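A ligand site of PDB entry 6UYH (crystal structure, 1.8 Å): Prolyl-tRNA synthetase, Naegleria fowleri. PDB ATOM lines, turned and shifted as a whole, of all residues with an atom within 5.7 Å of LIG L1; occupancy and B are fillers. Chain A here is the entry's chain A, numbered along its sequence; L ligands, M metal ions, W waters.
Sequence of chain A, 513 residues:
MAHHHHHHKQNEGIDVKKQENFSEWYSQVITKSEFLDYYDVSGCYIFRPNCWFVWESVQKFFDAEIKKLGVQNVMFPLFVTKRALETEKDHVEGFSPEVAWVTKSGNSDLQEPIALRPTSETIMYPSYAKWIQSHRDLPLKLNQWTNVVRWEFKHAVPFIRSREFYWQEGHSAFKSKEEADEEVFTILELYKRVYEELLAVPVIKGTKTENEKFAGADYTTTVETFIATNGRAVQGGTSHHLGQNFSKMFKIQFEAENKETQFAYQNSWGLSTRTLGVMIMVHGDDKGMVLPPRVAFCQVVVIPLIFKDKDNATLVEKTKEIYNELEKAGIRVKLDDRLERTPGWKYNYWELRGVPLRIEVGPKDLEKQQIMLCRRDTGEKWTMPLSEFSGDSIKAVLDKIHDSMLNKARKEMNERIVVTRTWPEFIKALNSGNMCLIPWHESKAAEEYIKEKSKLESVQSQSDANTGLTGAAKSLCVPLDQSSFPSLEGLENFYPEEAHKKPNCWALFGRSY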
ATOM      1  N   LEU A  85     -24.677 -15.455 -26.438  1.00  0.00           N
ATOM      2  CA  LEU A  85     -23.729 -16.423 -25.921  1.00  0.00           C
ATOM      3  C   LEU A  85     -22.382 -16.308 -26.605  1.00  0.00           C
ATOM      4  O   LEU A  85     -21.335 -16.339 -25.947  1.00  0.00           O
ATOM      5  CB  LEU A  85     -24.308 -17.825 -26.076  1.00  0.00           C
ATOM      6  CG  LEU A  85     -23.988 -18.935 -25.098  1.00  0.00           C
ATOM      7  CD1 LEU A  85     -24.162 -18.483 -23.659  1.00  0.00           C
ATOM      8  CD2 LEU A  85     -24.914 -20.106 -25.431  1.00  0.00           C
ATOM      9  N   GLU A  88     -18.917 -13.684 -26.064  1.00  0.00           N
ATOM     10  CA  GLU A  88     -17.684 -13.953 -25.331  1.00  0.00           C
ATOM     11  C   GLU A  88     -16.527 -14.355 -26.244  1.00  0.00           C
ATOM     12  O   GLU A  88     -16.376 -15.518 -26.575  1.00  0.00           O
ATOM     13  CB  GLU A  88     -17.921 -15.032 -24.284  1.00  0.00           C
ATOM     14  CG  GLU A  88     -18.081 -14.484 -22.878  1.00  0.00           C
ATOM     15  CD  GLU A  88     -18.543 -15.536 -21.899  1.00  0.00           C
ATOM     16  OE1 GLU A  88     -18.790 -16.679 -22.331  1.00  0.00           O
ATOM     17  OE2 GLU A  88     -18.674 -15.210 -20.704  1.00  0.00           O
ATOM     18  N   PHE A  95     -16.470 -24.164 -24.137  1.00  0.00           N
ATOM     19  CA  PHE A  95     -17.644 -24.623 -23.418  1.00  0.00           C
ATOM     20  C   PHE A  95     -18.781 -25.045 -24.336  1.00  0.00           C
ATOM     21  O   PHE A  95     -19.766 -25.622 -23.850  1.00  0.00           O
ATOM     22  CB  PHE A  95     -18.151 -23.522 -22.488  1.00  0.00           C
ATOM     23  CG  PHE A  95     -17.293 -23.271 -21.282  1.00  0.00           C
ATOM     24  CD1 PHE A  95     -17.013 -24.292 -20.390  1.00  0.00           C
ATOM     25  CD2 PHE A  95     -16.831 -21.993 -21.003  1.00  0.00           C
ATOM     26  CE1 PHE A  95     -16.243 -24.050 -19.255  1.00  0.00           C
ATOM     27  CE2 PHE A  95     -16.068 -21.744 -19.867  1.00  0.00           C
ATOM     28  CZ  PHE A  95     -15.765 -22.785 -19.004  1.00  0.00           C
ATOM     29  N   SER A  96     -18.658 -24.805 -25.644  1.00  0.00           N
ATOM     30  CA  SER A  96     -19.788 -25.004 -26.541  1.00  0.00           C
ATOM     31  C   SER A  96     -20.374 -26.420 -26.492  1.00  0.00           C
ATOM     32  O   SER A  96     -21.598 -26.542 -26.626  1.00  0.00           O
ATOM     33  CB  SER A  96     -19.387 -24.628 -27.976  1.00  0.00           C
ATOM     34  OG  SER A  96     -18.467 -25.542 -28.551  1.00  0.00           O
ATOM     35  N   GLU A  98     -21.027 -28.135 -23.941  1.00  0.00           N
ATOM     36  CA  GLU A  98     -21.854 -28.268 -22.744  1.00  0.00           C
ATOM     37  C   GLU A  98     -23.167 -27.486 -22.810  1.00  0.00           C
ATOM     38  O   GLU A  98     -23.968 -27.586 -21.878  1.00  0.00           O
ATOM     39  CB  GLU A  98     -21.078 -27.795 -21.502  1.00  0.00           C
ATOM     40  CG  GLU A  98     -19.872 -28.645 -21.130  1.00  0.00           C
ATOM     41  CD  GLU A  98     -19.308 -28.288 -19.747  1.00  0.00           C
ATOM     42  OE1 GLU A  98     -18.445 -29.035 -19.243  1.00  0.00           O
ATOM     43  OE2 GLU A  98     -19.730 -27.260 -19.153  1.00  0.00           O
ATOM     44  N   VAL A  99     -23.415 -26.727 -23.880  1.00  0.00           N
ATOM     45  CA  VAL A  99     -24.620 -25.899 -23.984  1.00  0.00           C
ATOM     46  C   VAL A  99     -25.797 -26.766 -24.425  1.00  0.00           C
ATOM     47  O   VAL A  99     -25.710 -27.476 -25.431  1.00  0.00           O
ATOM     48  CB  VAL A  99     -24.408 -24.749 -24.976  1.00  0.00           C
ATOM     49  CG1 VAL A  99     -25.625 -23.869 -24.998  1.00  0.00           C
ATOM     50  CG2 VAL A  99     -23.133 -23.952 -24.649  1.00  0.00           C
ATOM     51  N   PRO A 118     -26.232 -21.365 -18.889  1.00  0.00           N
ATOM     52  CA  PRO A 118     -25.141 -22.113 -18.230  1.00  0.00           C
ATOM     53  C   PRO A 118     -24.436 -21.278 -17.172  1.00  0.00           C
ATOM     54  O   PRO A 118     -23.603 -21.778 -16.406  1.00  0.00           O
ATOM     55  CB  PRO A 118     -24.199 -22.418 -19.395  1.00  0.00           C
ATOM     56  CG  PRO A 118     -24.328 -21.205 -20.275  1.00  0.00           C
ATOM     57  CD  PRO A 118     -25.766 -20.720 -20.133  1.00  0.00           C
ATOM     58  N   THR A 119     -24.771 -19.986 -17.182  1.00  0.00           N
ATOM     59  CA  THR A 119     -24.274 -18.886 -16.355  1.00  0.00           C
ATOM     60  C   THR A 119     -24.812 -17.633 -17.042  1.00  0.00           C
ATOM     61  O   THR A 119     -25.202 -17.717 -18.211  1.00  0.00           O
ATOM     62  CB  THR A 119     -22.741 -18.874 -16.211  1.00  0.00           C
ATOM     63  OG1 THR A 119     -22.367 -17.780 -15.357  1.00  0.00           O
ATOM     64  CG2 THR A 119     -22.069 -18.701 -17.577  1.00  0.00           C
ATOM     65  N   SER A 120     -24.876 -16.484 -16.358  1.00  0.00           N
ATOM     66  CA  SER A 120     -25.671 -15.377 -16.874  1.00  0.00           C
ATOM     67  C   SER A 120     -24.879 -14.138 -17.318  1.00  0.00           C
ATOM     68  O   SER A 120     -25.511 -13.094 -17.568  1.00  0.00           O
ATOM     69  CB  SER A 120     -26.731 -14.972 -15.856  1.00  0.00           C
ATOM     70  OG  SER A 120     -27.596 -16.066 -15.624  1.00  0.00           O
ATOM     71  N   GLU A 121     -23.554 -14.211 -17.465  1.00  0.00           N
ATOM     72  CA  GLU A 121     -22.803 -13.050 -17.933  1.00  0.00           C
ATOM     73  C   GLU A 121     -23.373 -12.480 -19.232  1.00  0.00           C
ATOM     74  O   GLU A 121     -23.587 -11.264 -19.341  1.00  0.00           O
ATOM     75  CB  GLU A 121     -21.329 -13.404 -18.140  1.00  0.00           C
ATOM     76  CG  GLU A 121     -20.490 -13.471 -16.872  1.00  0.00           C
ATOM     77  CD  GLU A 121     -20.611 -14.798 -16.139  1.00  0.00           C
ATOM     78  OE1 GLU A 121     -21.344 -15.692 -16.620  1.00  0.00           O
ATOM     79  OE2 GLU A 121     -19.961 -14.960 -15.090  1.00  0.00           O
ATOM     80  N   VAL A 149     -27.980 -25.068 -16.280  1.00  0.00           N
ATOM     81  CA  VAL A 149     -27.904 -26.296 -17.084  1.00  0.00           C
ATOM     82  C   VAL A 149     -26.560 -26.346 -17.783  1.00  0.00           C
ATOM     83  O   VAL A 149     -26.208 -25.430 -18.532  1.00  0.00           O
ATOM     84  CB  VAL A 149     -29.038 -26.386 -18.114  1.00  0.00           C
ATOM     85  CG1 VAL A 149     -28.855 -27.623 -19.005  1.00  0.00           C
ATOM     86  CG2 VAL A 149     -30.414 -26.420 -17.404  1.00  0.00           C
ATOM     87  N   ARG A 150     -25.828 -27.432 -17.560  1.00  0.00           N
ATOM     88  CA  ARG A 150     -24.598 -27.706 -18.314  1.00  0.00           C
ATOM     89  C   ARG A 150     -24.566 -29.180 -18.667  1.00  0.00           C
ATOM     90  O   ARG A 150     -24.707 -30.031 -17.785  1.00  0.00           O
ATOM     91  CB  ARG A 150     -23.348 -27.340 -17.501  1.00  0.00           C
ATOM     92  CG  ARG A 150     -23.259 -25.879 -17.114  1.00  0.00           C
ATOM     93  CD  ARG A 150     -22.144 -25.616 -16.112  1.00  0.00           C
ATOM     94  NE  ARG A 150     -22.118 -24.197 -15.754  1.00  0.00           N
ATOM     95  CZ  ARG A 150     -21.209 -23.641 -14.959  1.00  0.00           C
ATOM     96  NH1 ARG A 150     -20.237 -24.384 -14.434  1.00  0.00           N
ATOM     97  NH2 ARG A 150     -21.262 -22.346 -14.680  1.00  0.00           N
ATOM     98  N   TRP A 167     -27.955 -22.490  -7.886  1.00  0.00           N
ATOM     99  CA  TRP A 167     -26.899 -21.670  -7.320  1.00  0.00           C
ATOM    100  C   TRP A 167     -27.442 -20.279  -7.035  1.00  0.00           C
ATOM    101  O   TRP A 167     -28.607 -19.979  -7.298  1.00  0.00           O
ATOM    102  CB  TRP A 167     -25.662 -21.619  -8.237  1.00  0.00           C
ATOM    103  CG  TRP A 167     -25.733 -20.759  -9.507  1.00  0.00           C
ATOM    104  CD1 TRP A 167     -26.786 -20.010  -9.972  1.00  0.00           C
ATOM    105  CD2 TRP A 167     -24.684 -20.621 -10.470  1.00  0.00           C
ATOM    106  NE1 TRP A 167     -26.425 -19.395 -11.161  1.00  0.00           N
ATOM    107  CE2 TRP A 167     -25.146 -19.760 -11.486  1.00  0.00           C
ATOM    108  CE3 TRP A 167     -23.385 -21.140 -10.559  1.00  0.00           C
ATOM    109  CZ2 TRP A 167     -24.358 -19.409 -12.581  1.00  0.00           C
ATOM    110  CZ3 TRP A 167     -22.603 -20.794 -11.647  1.00  0.00           C
ATOM    111  CH2 TRP A 167     -23.095 -19.934 -12.644  1.00  0.00           C
ATOM    112  N   GLN A 168     -26.599 -19.437  -6.452  1.00  0.00           N
ATOM    113  CA  GLN A 168     -26.731 -17.996  -6.613  1.00  0.00           C
ATOM    114  C   GLN A 168     -25.557 -17.558  -7.463  1.00  0.00           C
ATOM    115  O   GLN A 168     -24.462 -18.107  -7.347  1.00  0.00           O
ATOM    116  CB  GLN A 168     -26.743 -17.228  -5.285  1.00  0.00           C
ATOM    117  CG  GLN A 168     -25.511 -17.451  -4.370  1.00  0.00           C
ATOM    118  CD  GLN A 168     -24.224 -16.710  -4.780  1.00  0.00           C
ATOM    119  OE1 GLN A 168     -23.113 -17.196  -4.501  1.00  0.00           O
ATOM    120  NE2 GLN A 168     -24.350 -15.531  -5.399  1.00  0.00           N
ATOM    121  N   GLU A 169     -25.793 -16.578  -8.334  1.00  0.00           N
ATOM    122  CA  GLU A 169     -24.719 -15.886  -9.024  1.00  0.00           C
ATOM    123  C   GLU A 169     -24.863 -14.389  -8.783  1.00  0.00           C
ATOM    124  O   GLU A 169     -25.944 -13.810  -8.988  1.00  0.00           O
ATOM    125  CB  GLU A 169     -24.694 -16.215 -10.539  1.00  0.00           C
ATOM    126  CG  GLU A 169     -26.010 -15.941 -11.263  1.00  0.00           C
ATOM    127  CD  GLU A 169     -25.960 -16.316 -12.731  1.00  0.00           C
ATOM    128  OE1 GLU A 169     -26.944 -16.911 -13.214  1.00  0.00           O
ATOM    129  OE2 GLU A 169     -24.947 -16.006 -13.388  1.00  0.00           O
ATOM    130  N   GLY A 170     -23.781 -13.771  -8.320  1.00  0.00           N
ATOM    131  CA  GLY A 170     -23.743 -12.337  -8.081  1.00  0.00           C
ATOM    132  C   GLY A 170     -22.858 -11.695  -9.143  1.00  0.00           C
ATOM    133  O   GLY A 170     -21.856 -12.271  -9.547  1.00  0.00           O
ATOM    134  N   HIS A 171     -23.274 -10.528  -9.602  1.00  0.00           N
ATOM    135  CA  HIS A 171     -22.593  -9.788 -10.668  1.00  0.00           C
ATOM    136  C   HIS A 171     -22.559  -8.325 -10.248  1.00  0.00           C
ATOM    137  O   HIS A 171     -23.621  -7.699 -10.142  1.00  0.00           O
ATOM    138  CB  HIS A 171     -23.310  -9.961 -12.014  1.00  0.00           C
ATOM    139  CG  HIS A 171     -23.368 -11.377 -12.495  1.00  0.00           C
ATOM    140  ND1 HIS A 171     -22.484 -11.864 -13.439  1.00  0.00           N
ATOM    141  CD2 HIS A 171     -24.184 -12.403 -12.161  1.00  0.00           C
ATOM    142  CE1 HIS A 171     -22.764 -13.140 -13.664  1.00  0.00           C
ATOM    143  NE2 HIS A 171     -23.785 -13.489 -12.904  1.00  0.00           N
ATOM    144  N   PHE A 214     -11.211 -18.665 -14.350  1.00  0.00           N
ATOM    145  CA  PHE A 214     -12.170 -18.311 -15.386  1.00  0.00           C
ATOM    146  C   PHE A 214     -11.469 -17.525 -16.488  1.00  0.00           C
ATOM    147  O   PHE A 214     -10.823 -16.499 -16.228  1.00  0.00           O
ATOM    148  CB  PHE A 214     -13.303 -17.499 -14.755  1.00  0.00           C
ATOM    149  CG  PHE A 214     -14.400 -17.071 -15.707  1.00  0.00           C
ATOM    150  CD1 PHE A 214     -15.101 -15.890 -15.471  1.00  0.00           C
ATOM    151  CD2 PHE A 214     -14.737 -17.839 -16.807  1.00  0.00           C
ATOM    152  CE1 PHE A 214     -16.125 -15.494 -16.322  1.00  0.00           C
ATOM    153  CE2 PHE A 214     -15.756 -17.437 -17.664  1.00  0.00           C
ATOM    154  CZ  PHE A 214     -16.444 -16.260 -17.421  1.00  0.00           C
ATOM    155  N   THR A 238     -16.789 -19.804  -5.828  1.00  0.00           N
ATOM    156  CA  THR A 238     -15.851 -19.094  -6.689  1.00  0.00           C
ATOM    157  C   THR A 238     -16.143 -17.602  -6.649  1.00  0.00           C
ATOM    158  O   THR A 238     -17.312 -17.204  -6.705  1.00  0.00           O
ATOM    159  CB  THR A 238     -15.966 -19.608  -8.122  1.00  0.00           C
ATOM    160  OG1 THR A 238     -15.917 -21.039  -8.121  1.00  0.00           O
ATOM    161  CG2 THR A 238     -14.820 -19.103  -8.939  1.00  0.00           C
ATOM    162  N   HIS A 240     -14.682 -14.116  -8.634  1.00  0.00           N
ATOM    163  CA  HIS A 240     -13.817 -13.601  -9.694  1.00  0.00           C
ATOM    164  C   HIS A 240     -13.734 -12.092  -9.637  1.00  0.00           C
ATOM    165  O   HIS A 240     -14.753 -11.416  -9.481  1.00  0.00           O
ATOM    166  CB  HIS A 240     -14.352 -13.944 -11.088  1.00  0.00           C
ATOM    167  CG  HIS A 240     -14.672 -15.378 -11.308  1.00  0.00           C
ATOM    168  ND1 HIS A 240     -13.692 -16.332 -11.514  1.00  0.00           N
ATOM    169  CD2 HIS A 240     -15.858 -16.021 -11.424  1.00  0.00           C
ATOM    170  CE1 HIS A 240     -14.261 -17.506 -11.705  1.00  0.00           C
ATOM    171  NE2 HIS A 240     -15.577 -17.341 -11.663  1.00  0.00           N
ATOM    172  N   SER A 268     -17.810 -11.306 -10.602  1.00  0.00           N
ATOM    173  CA  SER A 268     -18.932 -12.238 -10.477  1.00  0.00           C
ATOM    174  C   SER A 268     -18.531 -13.368  -9.538  1.00  0.00           C
ATOM    175  O   SER A 268     -17.350 -13.626  -9.320  1.00  0.00           O
ATOM    176  CB  SER A 268     -19.417 -12.781 -11.836  1.00  0.00           C
ATOM    177  OG  SER A 268     -18.439 -13.628 -12.430  1.00  0.00           O
ATOM    178  N   TRP A 269     -19.533 -14.019  -8.940  1.00  0.00           N
ATOM    179  CA  TRP A 269     -19.248 -14.987  -7.886  1.00  0.00           C
ATOM    180  C   TRP A 269     -20.449 -15.924  -7.774  1.00  0.00           C
ATOM    181  O   TRP A 269     -21.590 -15.495  -7.953  1.00  0.00           O
ATOM    182  CB  TRP A 269     -18.967 -14.293  -6.533  1.00  0.00           C
ATOM    183  CG  TRP A 269     -19.534 -12.866  -6.381  1.00  0.00           C
ATOM    184  CD1 TRP A 269     -18.934 -11.695  -6.786  1.00  0.00           C
ATOM    185  CD2 TRP A 269     -20.778 -12.479  -5.766  1.00  0.00           C
ATOM    186  NE1 TRP A 269     -19.734 -10.609  -6.465  1.00  0.00           N
ATOM    187  CE2 TRP A 269     -20.866 -11.068  -5.836  1.00  0.00           C
ATOM    188  CE3 TRP A 269     -21.821 -13.194  -5.148  1.00  0.00           C
ATOM    189  CZ2 TRP A 269     -21.957 -10.348  -5.324  1.00  0.00           C
ATOM    190  CZ3 TRP A 269     -22.911 -12.474  -4.636  1.00  0.00           C
ATOM    191  CH2 TRP A 269     -22.974 -11.066  -4.732  1.00  0.00           C
ATOM    192  N   GLY A 270     -20.180 -17.204  -7.511  1.00  0.00           N
ATOM    193  CA  GLY A 270     -21.266 -18.169  -7.430  1.00  0.00           C
ATOM    194  C   GLY A 270     -20.985 -19.262  -6.424  1.00  0.00           C
ATOM    195  O   GLY A 270     -19.842 -19.650  -6.191  1.00  0.00           O
HETATM  196  O1  LIG L   1     -19.808 -19.591 -14.925  1.00  0.00           O
HETATM  197  C1  LIG L   1     -18.637 -19.280 -14.961  1.00  0.00           C
HETATM  198  C2  LIG L   1     -18.129 -18.014 -14.318  1.00  0.00           C
HETATM  199  C3  LIG L   1     -18.964 -17.478 -13.146  1.00  0.00           C
HETATM  200  N1  LIG L   1     -20.296 -17.012 -13.561  1.00  0.00           N
HETATM  201  C4  LIG L   1     -21.017 -16.369 -12.465  1.00  0.00           C
HETATM  202  C5  LIG L   1     -21.205 -17.299 -11.295  1.00  0.00           C
HETATM  203  C6  LIG L   1     -19.862 -17.878 -10.839  1.00  0.00           C
HETATM  204  C7  LIG L   1     -19.122 -18.488 -12.017  1.00  0.00           C
HETATM  205  O2  LIG L   1     -17.834 -18.940 -11.582  1.00  0.00           O
HETATM  206  C8  LIG L   1     -17.605 -20.155 -15.690  1.00  0.00           C
HETATM  207  N2  LIG L   1     -18.228 -21.025 -16.689  1.00  0.00           N
HETATM  208  C9  LIG L   1     -18.751 -20.419 -17.817  1.00  0.00           C
HETATM  209  O3  LIG L   1     -18.660 -19.219 -18.002  1.00  0.00           O
HETATM  210  C10 LIG L   1     -19.442 -21.355 -18.727  1.00  0.00           C
HETATM  211  C11 LIG L   1     -20.008 -20.894 -19.907  1.00  0.00           C
HETATM  212  C12 LIG L   1     -18.347 -22.360 -16.454  1.00  0.00           C
HETATM  213  N3  LIG L   1     -18.956 -23.212 -17.202  1.00  0.00           N
HETATM  214  C13 LIG L   1     -19.540 -22.701 -18.371  1.00  0.00           C
HETATM  215  C14 LIG L   1     -20.257 -23.583 -19.178  1.00  0.00           C
HETATM  216  C15 LIG L   1     -20.843 -23.102 -20.343  1.00  0.00           C
HETATM  217 BR1  LIG L   1     -21.893 -24.292 -21.361  1.00  0.00          BR
HETATM  218  C16 LIG L   1     -20.689 -21.783 -20.719  1.00  0.00           C
HETATM  219 CL1  LIG L   1     -21.302 -21.205 -22.240  1.00  0.00          CL
HETATM  220  P1  LG2 L   2     -15.879 -27.359 -12.093  1.00  0.00           P
HETATM  221  O1  LG2 L   2     -14.506 -27.777 -12.333  1.00  0.00           O
HETATM  222  O2  LG2 L   2     -16.746 -27.793 -13.352  1.00  0.00           O
HETATM  223  O3  LG2 L   2     -16.345 -28.101 -10.773  1.00  0.00           O
HETATM  224  P2  LG2 L   2     -16.578 -24.545 -12.833  1.00  0.00           P
HETATM  225  O4  LG2 L   2     -15.522 -23.648 -13.285  1.00  0.00           O
HETATM  226  O5  LG2 L   2     -17.302 -25.160 -14.071  1.00  0.00           O
HETATM  227  N1  LG2 L   2     -16.014 -25.744 -11.855  1.00  0.00           N
HETATM  228  P3  LG2 L   2     -18.222 -22.310 -12.004  1.00  0.00           P
HETATM  229  O6  LG2 L   2     -17.207 -21.289 -11.686  1.00  0.00           O
HETATM  230  O7  LG2 L   2     -18.794 -22.079 -13.369  1.00  0.00           O
HETATM  231  O8  LG2 L   2     -17.627 -23.786 -11.981  1.00  0.00           O
HETATM  232  O9  LG2 L   2     -19.441 -22.430 -10.972  1.00  0.00           O
HETATM  233  C1  LG2 L   2     -19.562 -21.815  -9.664  1.00  0.00           C
HETATM  234  C2  LG2 L   2     -19.606 -22.920  -8.657  1.00  0.00           C
HETATM  235  O10 LG2 L   2     -20.695 -23.821  -8.955  1.00  0.00           O
HETATM  236  C3  LG2 L   2     -18.367 -23.806  -8.684  1.00  0.00           C
HETATM  237  O11 LG2 L   2     -17.337 -23.249  -7.874  1.00  0.00           O
HETATM  238  C4  LG2 L   2     -18.879 -25.132  -8.110  1.00  0.00           C
HETATM  239  O12 LG2 L   2     -18.751 -25.148  -6.689  1.00  0.00           O
HETATM  240  C5  LG2 L   2     -20.354 -25.148  -8.571  1.00  0.00           C
HETATM  241  N2  LG2 L   2     -20.611 -26.031  -9.698  1.00  0.00           N
HETATM  242  C6  LG2 L   2     -20.012 -26.011 -10.926  1.00  0.00           C
HETATM  243  N3  LG2 L   2     -20.439 -26.924 -11.753  1.00  0.00           N
HETATM  244  C7  LG2 L   2     -21.406 -27.603 -11.020  1.00  0.00           C
HETATM  245  C8  LG2 L   2     -22.233 -28.697 -11.326  1.00  0.00           C
HETATM  246  N4  LG2 L   2     -22.275 -29.288 -12.520  1.00  0.00           N
HETATM  247  N5  LG2 L   2     -23.059 -29.146 -10.350  1.00  0.00           N
HETATM  248  C9  LG2 L   2     -23.053 -28.534  -9.170  1.00  0.00           C
HETATM  249  N6  LG2 L   2     -22.328 -27.481  -8.767  1.00  0.00           N
HETATM  250  C10 LG2 L   2     -21.509 -27.065  -9.747  1.00  0.00           C
HETATM  251 MG    MG M   1     -17.607 -26.806 -15.192  1.00  0.00          MG
HETATM  252  O   HOH W   1     -19.612 -16.760 -19.081  1.00  0.00           O
HETATM  253  O   HOH W   2     -18.377 -25.879 -16.826  1.00  0.00           O
HETATM  254  O   HOH W   3     -14.650 -21.812 -15.520  1.00  0.00           O
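Water W2 lies within hydrogen-bond range of a nitrogen (N3) of LIG L1 (2.8 Å), the side-chain carboxylate (OE2) of Glu 98 (3.0 Å) and the guanidinium group (NH1) of Arg 150 (3.4 Å).
Phe 95 touches LIG L1.
CB of Glu 98 touches BR1 of LIG L1, at 3.6 Å.
Val 99 touches LIG L1.
Pro 118 touches LIG L1.
CH2 of Trp 167 touches C5 of LIG L1, 3.5 Å away.
Glu 169 touches LIG L1 (CB to C5, 3.7 Å).
CE1 of His 171 touches C4 of LIG L1, at 3.9 Å.
Phe 214 touches LIG L1 (CE2 to O3, 3.4 Å).
Thr 238 touches LIG L1 (CB to O2, 3.99 Å).
Ser 268 touches LIG L1 (OG to C4, 3.8 Å).
C of Trp 269 touches C6 of LIG L1, at 3.7 Å.
Gly 270 touches LIG L1 (N to C6, 3.4 Å).
Hydrophobic or aromatic side chains that line LIG L1: Phe 95, Val 99, Pro 118, Trp 167, His 171, Phe 214 and His 240.
Of the 23 residues printed, 16 come within 4 Å of LIG L1.
O6 of LG2 L2 sits at hydrogen-bond distance from O2 of LIG L1 (2.4 Å).
OE2 of Glu 121 lies within salt-bridge range of N1 of LIG L1, at 2.6 Å.
A ring nitrogen (NE2) of His 240 lies within hydrogen-bond range of an oxygen (O2) of LIG L1 (2.8 Å).
A nitrogen (N1) of LIG L1 lies within hydrogen-bond range of the side-chain hydroxyl (OG1) of Thr 119 (2.8 Å).
NH2 of Arg 150 lies within hydrogen-bond range of O1 of LIG L1, at 3.1 Å.
An oxygen (O7) of LG2 L2 is in salt-bridge range of the guanidinium group (NH2) of Arg 150, 2.8 Å away.
An oxygen (O11) of LG2 L2 sits at hydrogen-bond distance from the side-chain hydroxyl (OG1) of Thr 238 (2.6 Å).
The side-chain carboxylate (OE1) of Glu 121 is in hydrogen-bond range of the side-chain hydroxyl (OG1) of Thr 119, 2.6 Å away.
OE2 of Glu 121 lies within hydrogen-bond range of OG of Ser 268, 3.3 Å away.
The backbone NH (N) of His 240 sits at hydrogen-bond distance from the backbone carbonyl oxygen (O) of Ser 268 (2.8 Å).
The guanidinium group (NE) of Arg 150 lies within hydrogen-bond range of the backbone carbonyl oxygen (O) of Pro 118, 2.9 Å away.
N of Gly 270 sits at hydrogen-bond distance from O of Thr 238 (3.0 Å).
NE1 of Trp 167 lies within hydrogen-bond range of OE1 of Glu 169 (3.3 Å).
The backbone carbonyl oxygen (O) of Trp 269 lies within hydrogen-bond range of the backbone NH (N) of Gly 170 (2.8 Å).
The side-chain carboxylate (OE2) of Glu 169 sits at hydrogen-bond distance from a ring nitrogen (NE2) of His 171 (2.8 Å).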
